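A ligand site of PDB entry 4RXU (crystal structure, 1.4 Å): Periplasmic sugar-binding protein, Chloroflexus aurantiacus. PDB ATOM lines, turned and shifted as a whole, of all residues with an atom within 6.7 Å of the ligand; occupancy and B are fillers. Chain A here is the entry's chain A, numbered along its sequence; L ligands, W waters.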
ATOM      1  N   THR A  39      15.536   1.982   6.167  1.00  0.00           N
ATOM      2  CA  THR A  39      16.835   1.506   5.709  1.00  0.00           C
ATOM      3  C   THR A  39      17.947   2.262   6.398  1.00  0.00           C
ATOM      4  O   THR A  39      17.778   3.445   6.713  1.00  0.00           O
ATOM      5  CB  THR A  39      16.980   1.637   4.164  1.00  0.00           C
ATOM      6  OG1 THR A  39      18.266   1.141   3.752  1.00  0.00           O
ATOM      7  CG2 THR A  39      16.827   3.064   3.695  1.00  0.00           C
ATOM      8  N   GLU A  42      20.241   4.929   3.542  1.00  0.00           N
ATOM      9  CA  GLU A  42      19.975   6.350   3.311  1.00  0.00           C
ATOM     10  C   GLU A  42      20.393   7.068   4.578  1.00  0.00           C
ATOM     11  O   GLU A  42      19.900   6.731   5.643  1.00  0.00           O
ATOM     12  CB  GLU A  42      18.487   6.609   3.027  1.00  0.00           C
ATOM     13  CG  GLU A  42      17.970   5.983   1.725  1.00  0.00           C
ATOM     14  CD  GLU A  42      16.465   6.017   1.589  1.00  0.00           C
ATOM     15  OE1 GLU A  42      15.774   6.845   2.257  1.00  0.00           O
ATOM     16  OE2 GLU A  42      15.960   5.206   0.776  1.00  0.00           O
ATOM     17  N   PRO A  43      21.309   8.035   4.464  1.00  0.00           N
ATOM     18  CA  PRO A  43      21.883   8.609   5.703  1.00  0.00           C
ATOM     19  C   PRO A  43      20.859   9.213   6.664  1.00  0.00           C
ATOM     20  O   PRO A  43      21.049   9.223   7.873  1.00  0.00           O
ATOM     21  CB  PRO A  43      22.807   9.709   5.182  1.00  0.00           C
ATOM     22  CG  PRO A  43      23.232   9.226   3.851  1.00  0.00           C
ATOM     23  CD  PRO A  43      22.121   8.395   3.283  1.00  0.00           C
ATOM     24  N   ARG A  44      19.753   9.721   6.116  1.00  0.00           N
ATOM     25  CA  ARG A  44      18.736  10.401   6.895  1.00  0.00           C
ATOM     26  C   ARG A  44      18.354   9.582   8.124  1.00  0.00           C
ATOM     27  O   ARG A  44      18.278  10.130   9.224  1.00  0.00           O
ATOM     28  CB  ARG A  44      17.480  10.687   6.054  1.00  0.00           C
ATOM     29  CG  ARG A  44      16.237  11.093   6.835  1.00  0.00           C
ATOM     30  CD  ARG A  44      16.402  12.329   7.705  1.00  0.00           C
ATOM     31  NE  ARG A  44      15.339  12.327   8.704  1.00  0.00           N
ATOM     32  CZ  ARG A  44      14.077  12.721   8.519  1.00  0.00           C
ATOM     33  NH1 ARG A  44      13.187  12.538   9.496  1.00  0.00           N
ATOM     34  NH2 ARG A  44      13.680  13.293   7.389  1.00  0.00           N
ATOM     35  N   TRP A  45      18.142   8.275   7.934  1.00  0.00           N
ATOM     36  CA  TRP A  45      17.577   7.459   9.018  1.00  0.00           C
ATOM     37  C   TRP A  45      18.545   7.184  10.153  1.00  0.00           C
ATOM     38  O   TRP A  45      18.126   6.856  11.245  1.00  0.00           O
ATOM     39  CB  TRP A  45      16.897   6.174   8.511  1.00  0.00           C
ATOM     40  CG  TRP A  45      16.054   6.551   7.345  1.00  0.00           C
ATOM     41  CD1 TRP A  45      16.283   6.229   6.058  1.00  0.00           C
ATOM     42  CD2 TRP A  45      14.968   7.496   7.340  1.00  0.00           C
ATOM     43  NE1 TRP A  45      15.398   6.890   5.229  1.00  0.00           N
ATOM     44  CE2 TRP A  45      14.576   7.666   6.001  1.00  0.00           C
ATOM     45  CE3 TRP A  45      14.275   8.191   8.324  1.00  0.00           C
ATOM     46  CZ2 TRP A  45      13.556   8.521   5.629  1.00  0.00           C
ATOM     47  CZ3 TRP A  45      13.258   9.037   7.956  1.00  0.00           C
ATOM     48  CH2 TRP A  45      12.907   9.191   6.631  1.00  0.00           C
ATOM     49  N   CYS A  93       8.193   4.622   9.681  1.00  0.00           N
ATOM     50  CA  CYS A  93       8.539   5.291   8.464  1.00  0.00           C
ATOM     51  C   CYS A  93       8.619   4.239   7.347  1.00  0.00           C
ATOM     52  O   CYS A  93       9.520   3.416   7.344  1.00  0.00           O
ATOM     53  CB  CYS A  93       9.837   6.050   8.597  1.00  0.00           C
ATOM     54  SG  CYS A  93      10.326   6.809   7.049  1.00  0.00           S
ATOM     55  N   ASP A 118       7.587  10.635   9.393  1.00  0.00           N
ATOM     56  CA  ASP A 118       8.299  11.331   8.324  1.00  0.00           C
ATOM     57  C   ASP A 118       7.641  11.140   6.960  1.00  0.00           C
ATOM     58  O   ASP A 118       7.365  12.118   6.279  1.00  0.00           O
ATOM     59  CB  ASP A 118       9.779  10.978   8.227  1.00  0.00           C
ATOM     60  CG  ASP A 118      10.497  11.929   7.325  1.00  0.00           C
ATOM     61  OD1 ASP A 118      10.865  13.023   7.824  1.00  0.00           O
ATOM     62  OD2 ASP A 118      10.623  11.637   6.103  1.00  0.00           O
ATOM     63  N   ARG A 119       7.468   9.882   6.554  1.00  0.00           N
ATOM     64  CA  ARG A 119       6.827   9.514   5.296  1.00  0.00           C
ATOM     65  C   ARG A 119       5.473   8.950   5.596  1.00  0.00           C
ATOM     66  O   ARG A 119       5.259   8.335   6.654  1.00  0.00           O
ATOM     67  CB  ARG A 119       7.624   8.437   4.565  1.00  0.00           C
ATOM     68  CG  ARG A 119       9.005   8.850   4.171  1.00  0.00           C
ATOM     69  CD  ARG A 119       9.749   7.663   3.597  1.00  0.00           C
ATOM     70  NE  ARG A 119      11.040   8.038   3.082  1.00  0.00           N
ATOM     71  CZ  ARG A 119      11.950   7.185   2.650  1.00  0.00           C
ATOM     72  NH1 ARG A 119      11.727   5.877   2.726  1.00  0.00           N
ATOM     73  NH2 ARG A 119      13.095   7.631   2.169  1.00  0.00           N
ATOM     74  N   PHE A 133       7.692  16.682   8.847  1.00  0.00           N
ATOM     75  CA  PHE A 133       8.083  18.031   8.497  1.00  0.00           C
ATOM     76  C   PHE A 133       7.164  18.575   7.418  1.00  0.00           C
ATOM     77  O   PHE A 133       6.435  17.843   6.741  1.00  0.00           O
ATOM     78  CB  PHE A 133       9.519  18.090   8.005  1.00  0.00           C
ATOM     79  CG  PHE A 133      10.528  17.662   9.031  1.00  0.00           C
ATOM     80  CD1 PHE A 133      10.791  18.443  10.145  1.00  0.00           C
ATOM     81  CD2 PHE A 133      11.227  16.466   8.870  1.00  0.00           C
ATOM     82  CE1 PHE A 133      11.730  18.052  11.059  1.00  0.00           C
ATOM     83  CE2 PHE A 133      12.172  16.079   9.789  1.00  0.00           C
ATOM     84  CZ  PHE A 133      12.414  16.879  10.881  1.00  0.00           C
ATOM     85  N   SER A 135       6.805  19.155   4.161  1.00  0.00           N
ATOM     86  CA  SER A 135       7.525  18.766   2.944  1.00  0.00           C
ATOM     87  C   SER A 135       7.265  19.641   1.726  1.00  0.00           C
ATOM     88  O   SER A 135       8.182  19.834   0.897  1.00  0.00           O
ATOM     89  CB  SER A 135       7.236  17.312   2.576  1.00  0.00           C
ATOM     90  OG  SER A 135       7.718  16.422   3.563  1.00  0.00           O
ATOM     91  N   ASP A 166       8.508   6.879  -2.176  1.00  0.00           N
ATOM     92  CA  ASP A 166       8.424   7.807  -1.034  1.00  0.00           C
ATOM     93  C   ASP A 166       7.425   8.896  -1.361  1.00  0.00           C
ATOM     94  O   ASP A 166       7.653   9.697  -2.264  1.00  0.00           O
ATOM     95  CB  ASP A 166       9.818   8.409  -0.833  1.00  0.00           C
ATOM     96  CG  ASP A 166       9.897   9.403   0.275  1.00  0.00           C
ATOM     97  OD1 ASP A 166       8.892   9.616   0.985  1.00  0.00           O
ATOM     98  OD2 ASP A 166      11.023   9.944   0.425  1.00  0.00           O
ATOM     99  N   ASN A 167       6.304   8.952  -0.657  1.00  0.00           N
ATOM    100  CA  ASN A 167       5.350  10.036  -0.914  1.00  0.00           C
ATOM    101  C   ASN A 167       5.991  11.419  -0.785  1.00  0.00           C
ATOM    102  O   ASN A 167       5.576  12.383  -1.430  1.00  0.00           O
ATOM    103  CB  ASN A 167       4.155   9.916   0.018  1.00  0.00           C
ATOM    104  CG  ASN A 167       3.055  10.868  -0.332  1.00  0.00           C
ATOM    105  OD1 ASN A 167       2.492  10.817  -1.432  1.00  0.00           O
ATOM    106  ND2 ASN A 167       2.700  11.723   0.620  1.00  0.00           N
ATOM    107  N   ASN A 168       6.970  11.539   0.104  1.00  0.00           N
ATOM    108  CA  ASN A 168       7.635  12.836   0.251  1.00  0.00           C
ATOM    109  C   ASN A 168       8.315  13.273  -1.036  1.00  0.00           C
ATOM    110  O   ASN A 168       8.435  14.461  -1.261  1.00  0.00           O
ATOM    111  CB  ASN A 168       8.676  12.801   1.383  1.00  0.00           C
ATOM    112  CG  ASN A 168       8.061  12.758   2.752  1.00  0.00           C
ATOM    113  OD1 ASN A 168       6.887  13.032   2.939  1.00  0.00           O
ATOM    114  ND2 ASN A 168       8.895  12.463   3.735  1.00  0.00           N
ATOM    115  N   ALA A 169       8.775  12.339  -1.866  1.00  0.00           N
ATOM    116  CA  ALA A 169       9.400  12.714  -3.129  1.00  0.00           C
ATOM    117  C   ALA A 169       8.412  13.512  -3.988  1.00  0.00           C
ATOM    118  O   ALA A 169       8.789  14.461  -4.645  1.00  0.00           O
ATOM    119  CB  ALA A 169       9.929  11.505  -3.861  1.00  0.00           C
ATOM    120  N   PHE A 172       7.999  17.010  -2.149  1.00  0.00           N
ATOM    121  CA  PHE A 172       9.128  17.891  -2.382  1.00  0.00           C
ATOM    122  C   PHE A 172       9.080  18.406  -3.825  1.00  0.00           C
ATOM    123  O   PHE A 172       9.382  19.551  -4.095  1.00  0.00           O
ATOM    124  CB  PHE A 172      10.459  17.187  -2.190  1.00  0.00           C
ATOM    125  CG  PHE A 172      10.677  16.600  -0.826  1.00  0.00           C
ATOM    126  CD1 PHE A 172      10.313  17.251   0.349  1.00  0.00           C
ATOM    127  CD2 PHE A 172      11.336  15.402  -0.736  1.00  0.00           C
ATOM    128  CE1 PHE A 172      10.558  16.657   1.587  1.00  0.00           C
ATOM    129  CE2 PHE A 172      11.596  14.823   0.473  1.00  0.00           C
ATOM    130  CZ  PHE A 172      11.210  15.444   1.644  1.00  0.00           C
ATOM    131  N   TRP A 222      17.021   8.283  -4.167  1.00  0.00           N
ATOM    132  CA  TRP A 222      17.647   8.603  -2.876  1.00  0.00           C
ATOM    133  C   TRP A 222      18.980   7.885  -2.694  1.00  0.00           C
ATOM    134  O   TRP A 222      19.340   7.422  -1.599  1.00  0.00           O
ATOM    135  CB  TRP A 222      16.715   8.279  -1.715  1.00  0.00           C
ATOM    136  CG  TRP A 222      15.453   9.038  -1.587  1.00  0.00           C
ATOM    137  CD1 TRP A 222      14.226   8.511  -1.256  1.00  0.00           C
ATOM    138  CD2 TRP A 222      15.270  10.466  -1.631  1.00  0.00           C
ATOM    139  NE1 TRP A 222      13.289   9.526  -1.130  1.00  0.00           N
ATOM    140  CE2 TRP A 222      13.902  10.728  -1.363  1.00  0.00           C
ATOM    141  CE3 TRP A 222      16.125  11.545  -1.871  1.00  0.00           C
ATOM    142  CZ2 TRP A 222      13.388  12.020  -1.315  1.00  0.00           C
ATOM    143  CZ3 TRP A 222      15.594  12.832  -1.852  1.00  0.00           C
ATOM    144  CH2 TRP A 222      14.243  13.062  -1.564  1.00  0.00           C
ATOM    145  N   PRO A 251      17.393  16.978  -4.596  1.00  0.00           N
ATOM    146  CA  PRO A 251      16.303  16.806  -3.615  1.00  0.00           C
ATOM    147  C   PRO A 251      16.751  16.600  -2.179  1.00  0.00           C
ATOM    148  O   PRO A 251      16.010  16.887  -1.271  1.00  0.00           O
ATOM    149  CB  PRO A 251      15.545  15.584  -4.162  1.00  0.00           C
ATOM    150  CG  PRO A 251      16.595  14.791  -4.883  1.00  0.00           C
ATOM    151  CD  PRO A 251      17.478  15.836  -5.519  1.00  0.00           C
ATOM    152  N   ASN A 252      17.969  16.094  -1.966  1.00  0.00           N
ATOM    153  CA  ASN A 252      18.487  16.028  -0.592  1.00  0.00           C
ATOM    154  C   ASN A 252      19.984  16.186  -0.584  1.00  0.00           C
ATOM    155  O   ASN A 252      20.582  16.340  -1.625  1.00  0.00           O
ATOM    156  CB  ASN A 252      18.038  14.747   0.148  1.00  0.00           C
ATOM    157  CG  ASN A 252      18.813  13.507  -0.239  1.00  0.00           C
ATOM    158  OD1 ASN A 252      19.572  13.476  -1.216  1.00  0.00           O
ATOM    159  ND2 ASN A 252      18.587  12.430   0.521  1.00  0.00           N
ATOM    160  N   ASP A 253      20.593  16.117   0.600  1.00  0.00           N
ATOM    161  CA  ASP A 253      22.031  16.416   0.728  1.00  0.00           C
ATOM    162  C   ASP A 253      22.961  15.453  -0.002  1.00  0.00           C
ATOM    163  O   ASP A 253      23.842  15.885  -0.757  1.00  0.00           O
ATOM    164  CB  ASP A 253      22.420  16.525   2.193  1.00  0.00           C
ATOM    165  CG  ASP A 253      22.021  17.861   2.785  1.00  0.00           C
ATOM    166  OD1 ASP A 253      21.622  18.773   2.023  1.00  0.00           O
ATOM    167  OD2 ASP A 253      22.187  18.036   4.005  1.00  0.00           O
ATOM    168  N   GLN A 277      18.664  18.982   1.303  1.00  0.00           N
ATOM    169  CA  GLN A 277      17.983  18.968   2.593  1.00  0.00           C
ATOM    170  C   GLN A 277      18.562  17.876   3.476  1.00  0.00           C
ATOM    171  O   GLN A 277      19.139  16.925   2.978  1.00  0.00           O
ATOM    172  CB  GLN A 277      16.479  18.723   2.452  1.00  0.00           C
ATOM    173  CG  GLN A 277      16.096  17.306   2.047  1.00  0.00           C
ATOM    174  CD  GLN A 277      14.605  17.126   1.979  1.00  0.00           C
ATOM    175  OE1 GLN A 277      13.907  17.253   2.987  1.00  0.00           O
ATOM    176  NE2 GLN A 277      14.100  16.854   0.782  1.00  0.00           N
ATOM    177  N   ASP A 278      18.365  18.101   4.777  1.00  0.00           N
ATOM    178  CA  ASP A 278      18.671  17.182   5.906  1.00  0.00           C
ATOM    179  C   ASP A 278      19.852  17.684   6.745  1.00  0.00           C
ATOM    180  O   ASP A 278      20.077  17.174   7.844  1.00  0.00           O
ATOM    181  CB  ASP A 278      18.977  15.744   5.461  1.00  0.00           C
ATOM    182  CG  ASP A 278      17.786  15.028   4.818  1.00  0.00           C
ATOM    183  OD1 ASP A 278      16.628  15.472   4.917  1.00  0.00           O
ATOM    184  OD2 ASP A 278      18.043  13.947   4.243  1.00  0.00           O
ATOM    185  N   GLU A 280      22.957  17.097   6.466  1.00  0.00           N
ATOM    186  CA  GLU A 280      23.972  16.083   6.688  1.00  0.00           C
ATOM    187  C   GLU A 280      25.333  16.781   6.874  1.00  0.00           C
ATOM    188  O   GLU A 280      25.620  17.769   6.210  1.00  0.00           O
ATOM    189  CB  GLU A 280      24.011  15.090   5.526  1.00  0.00           C
ATOM    190  CG  GLU A 280      22.725  14.232   5.416  1.00  0.00           C
ATOM    191  CD  GLU A 280      22.514  13.206   6.528  1.00  0.00           C
ATOM    192  OE1 GLU A 280      23.503  12.844   7.225  1.00  0.00           O
ATOM    193  OE2 GLU A 280      21.374  12.731   6.702  1.00  0.00           O
ATOM    194  N   LYS A 298      15.850  20.295   8.701  1.00  0.00           N
ATOM    195  CA  LYS A 298      14.668  19.681   9.292  1.00  0.00           C
ATOM    196  C   LYS A 298      15.088  19.142  10.660  1.00  0.00           C
ATOM    197  O   LYS A 298      15.881  18.196  10.735  1.00  0.00           O
ATOM    198  CB  LYS A 298      14.123  18.577   8.380  1.00  0.00           C
ATOM    199  CG  LYS A 298      14.040  18.981   6.905  1.00  0.00           C
ATOM    200  CD  LYS A 298      13.130  18.138   6.045  1.00  0.00           C
ATOM    201  CE  LYS A 298      13.505  16.677   6.093  1.00  0.00           C
ATOM    202  NZ  LYS A 298      12.743  15.952   5.028  1.00  0.00           N
HETATM  203  C1  LIG L   1      13.106  12.252   3.965  1.00  0.00           C
HETATM  204  C2  LIG L   1      14.358  13.033   3.612  1.00  0.00           C
HETATM  205  C3  LIG L   1      15.434  12.057   3.143  1.00  0.00           C
HETATM  206  C4  LIG L   1      14.910  11.149   2.034  1.00  0.00           C
HETATM  207  C5  LIG L   1      15.888  10.063   1.639  1.00  0.00           C
HETATM  208  C6  LIG L   1      12.724  11.557   2.674  1.00  0.00           C
HETATM  209  O1  LIG L   1      11.455  10.965   2.727  1.00  0.00           O
HETATM  210  O2  LIG L   1      12.087  13.163   4.398  1.00  0.00           O
HETATM  211  O3  LIG L   1      14.771  13.733   4.779  1.00  0.00           O
HETATM  212  O4  LIG L   1      16.514  12.828   2.575  1.00  0.00           O
HETATM  213  O5  LIG L   1      13.700  10.537   2.421  1.00  0.00           O
HETATM  214  O6  LIG L   1      16.377   9.354   2.776  1.00  0.00           O
HETATM  215  O   HOH W   1      19.010  10.072   3.147  1.00  0.00           O
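O1 of the ligand lies within hydrogen-bond range of OD2 of Asp 166 (2.6 Å). O6 of the ligand is in hydrogen-bond range of OE1 of Glu 42, at 2.6 Å. The side-chain amide nitrogen (ND2) of Asn 168 sits at hydrogen-bond distance from an oxygen (O1) of the ligand (3.1 Å). An oxygen (O4) of the ligand lies within hydrogen-bond range of the side-chain amide nitrogen (ND2) of Asn 252. An oxygen (O4) of the ligand sits at hydrogen-bond distance from the side-chain carboxylate (OD2) of Asp 278. An oxygen (O2) of the ligand sits at hydrogen-bond distance from the side-chain amino group of Lys 298 (2.9 Å). NH2 of Arg 119 sits at hydrogen-bond distance from O5 of the ligand (3.0 Å). O2 of the ligand sits at hydrogen-bond distance from OD2 of Asp 118, at 2.7 Å. An oxygen (O3) of the ligand lies within hydrogen-bond range of the guanidinium group (NH2) of Arg 44, at 2.9 Å.
The side-chain amide nitrogen (ND2) of Asn 168 sits at hydrogen-bond distance from the backbone carbonyl oxygen (O) of Asp 118. The indole nitrogen (NE1) of Trp 222 lies within hydrogen-bond range of the side-chain carboxylate (OD2) of Asp 166 (2.8 Å). The guanidinium group (NH2) of Arg 44 is in salt-bridge range of the side-chain carboxylate (OD1) of Asp 118. OE1 of Glu 42 is in salt-bridge range of NH2 of Arg 119, 2.8 Å away. The side-chain carboxylate (OD2) of Asp 166 is in salt-bridge range of the guanidinium group (NE) of Arg 119 (3.3 Å). OD1 of Asp 166 is in hydrogen-bond range of N of Asn 168 (2.9 Å). The side-chain amino group of Lys 298 is in hydrogen-bond range of the side-chain amide oxygen of Gln 277 (2.7 Å). NE1 of Trp 45 lies within hydrogen-bond range of OE1 of Glu 42 (3.0 Å).
Trp 45 touches the ligand. CZ of Phe 172 touches O2 of the ligand, 3.7 Å away. CD2 of Trp 222 touches C5 of the ligand, at 3.4 Å. Within 4 Å of the ligand: Glu 42, Arg 44, Trp 45, Asp 118, Arg 119, Asp 166, Asn 168, Phe 172, Trp 222, Asn 252, Asp 278 and Lys 298.
Water W1 bridges O6 of the ligand (2.8 Å) and N of Arg 44 (3.1 Å).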
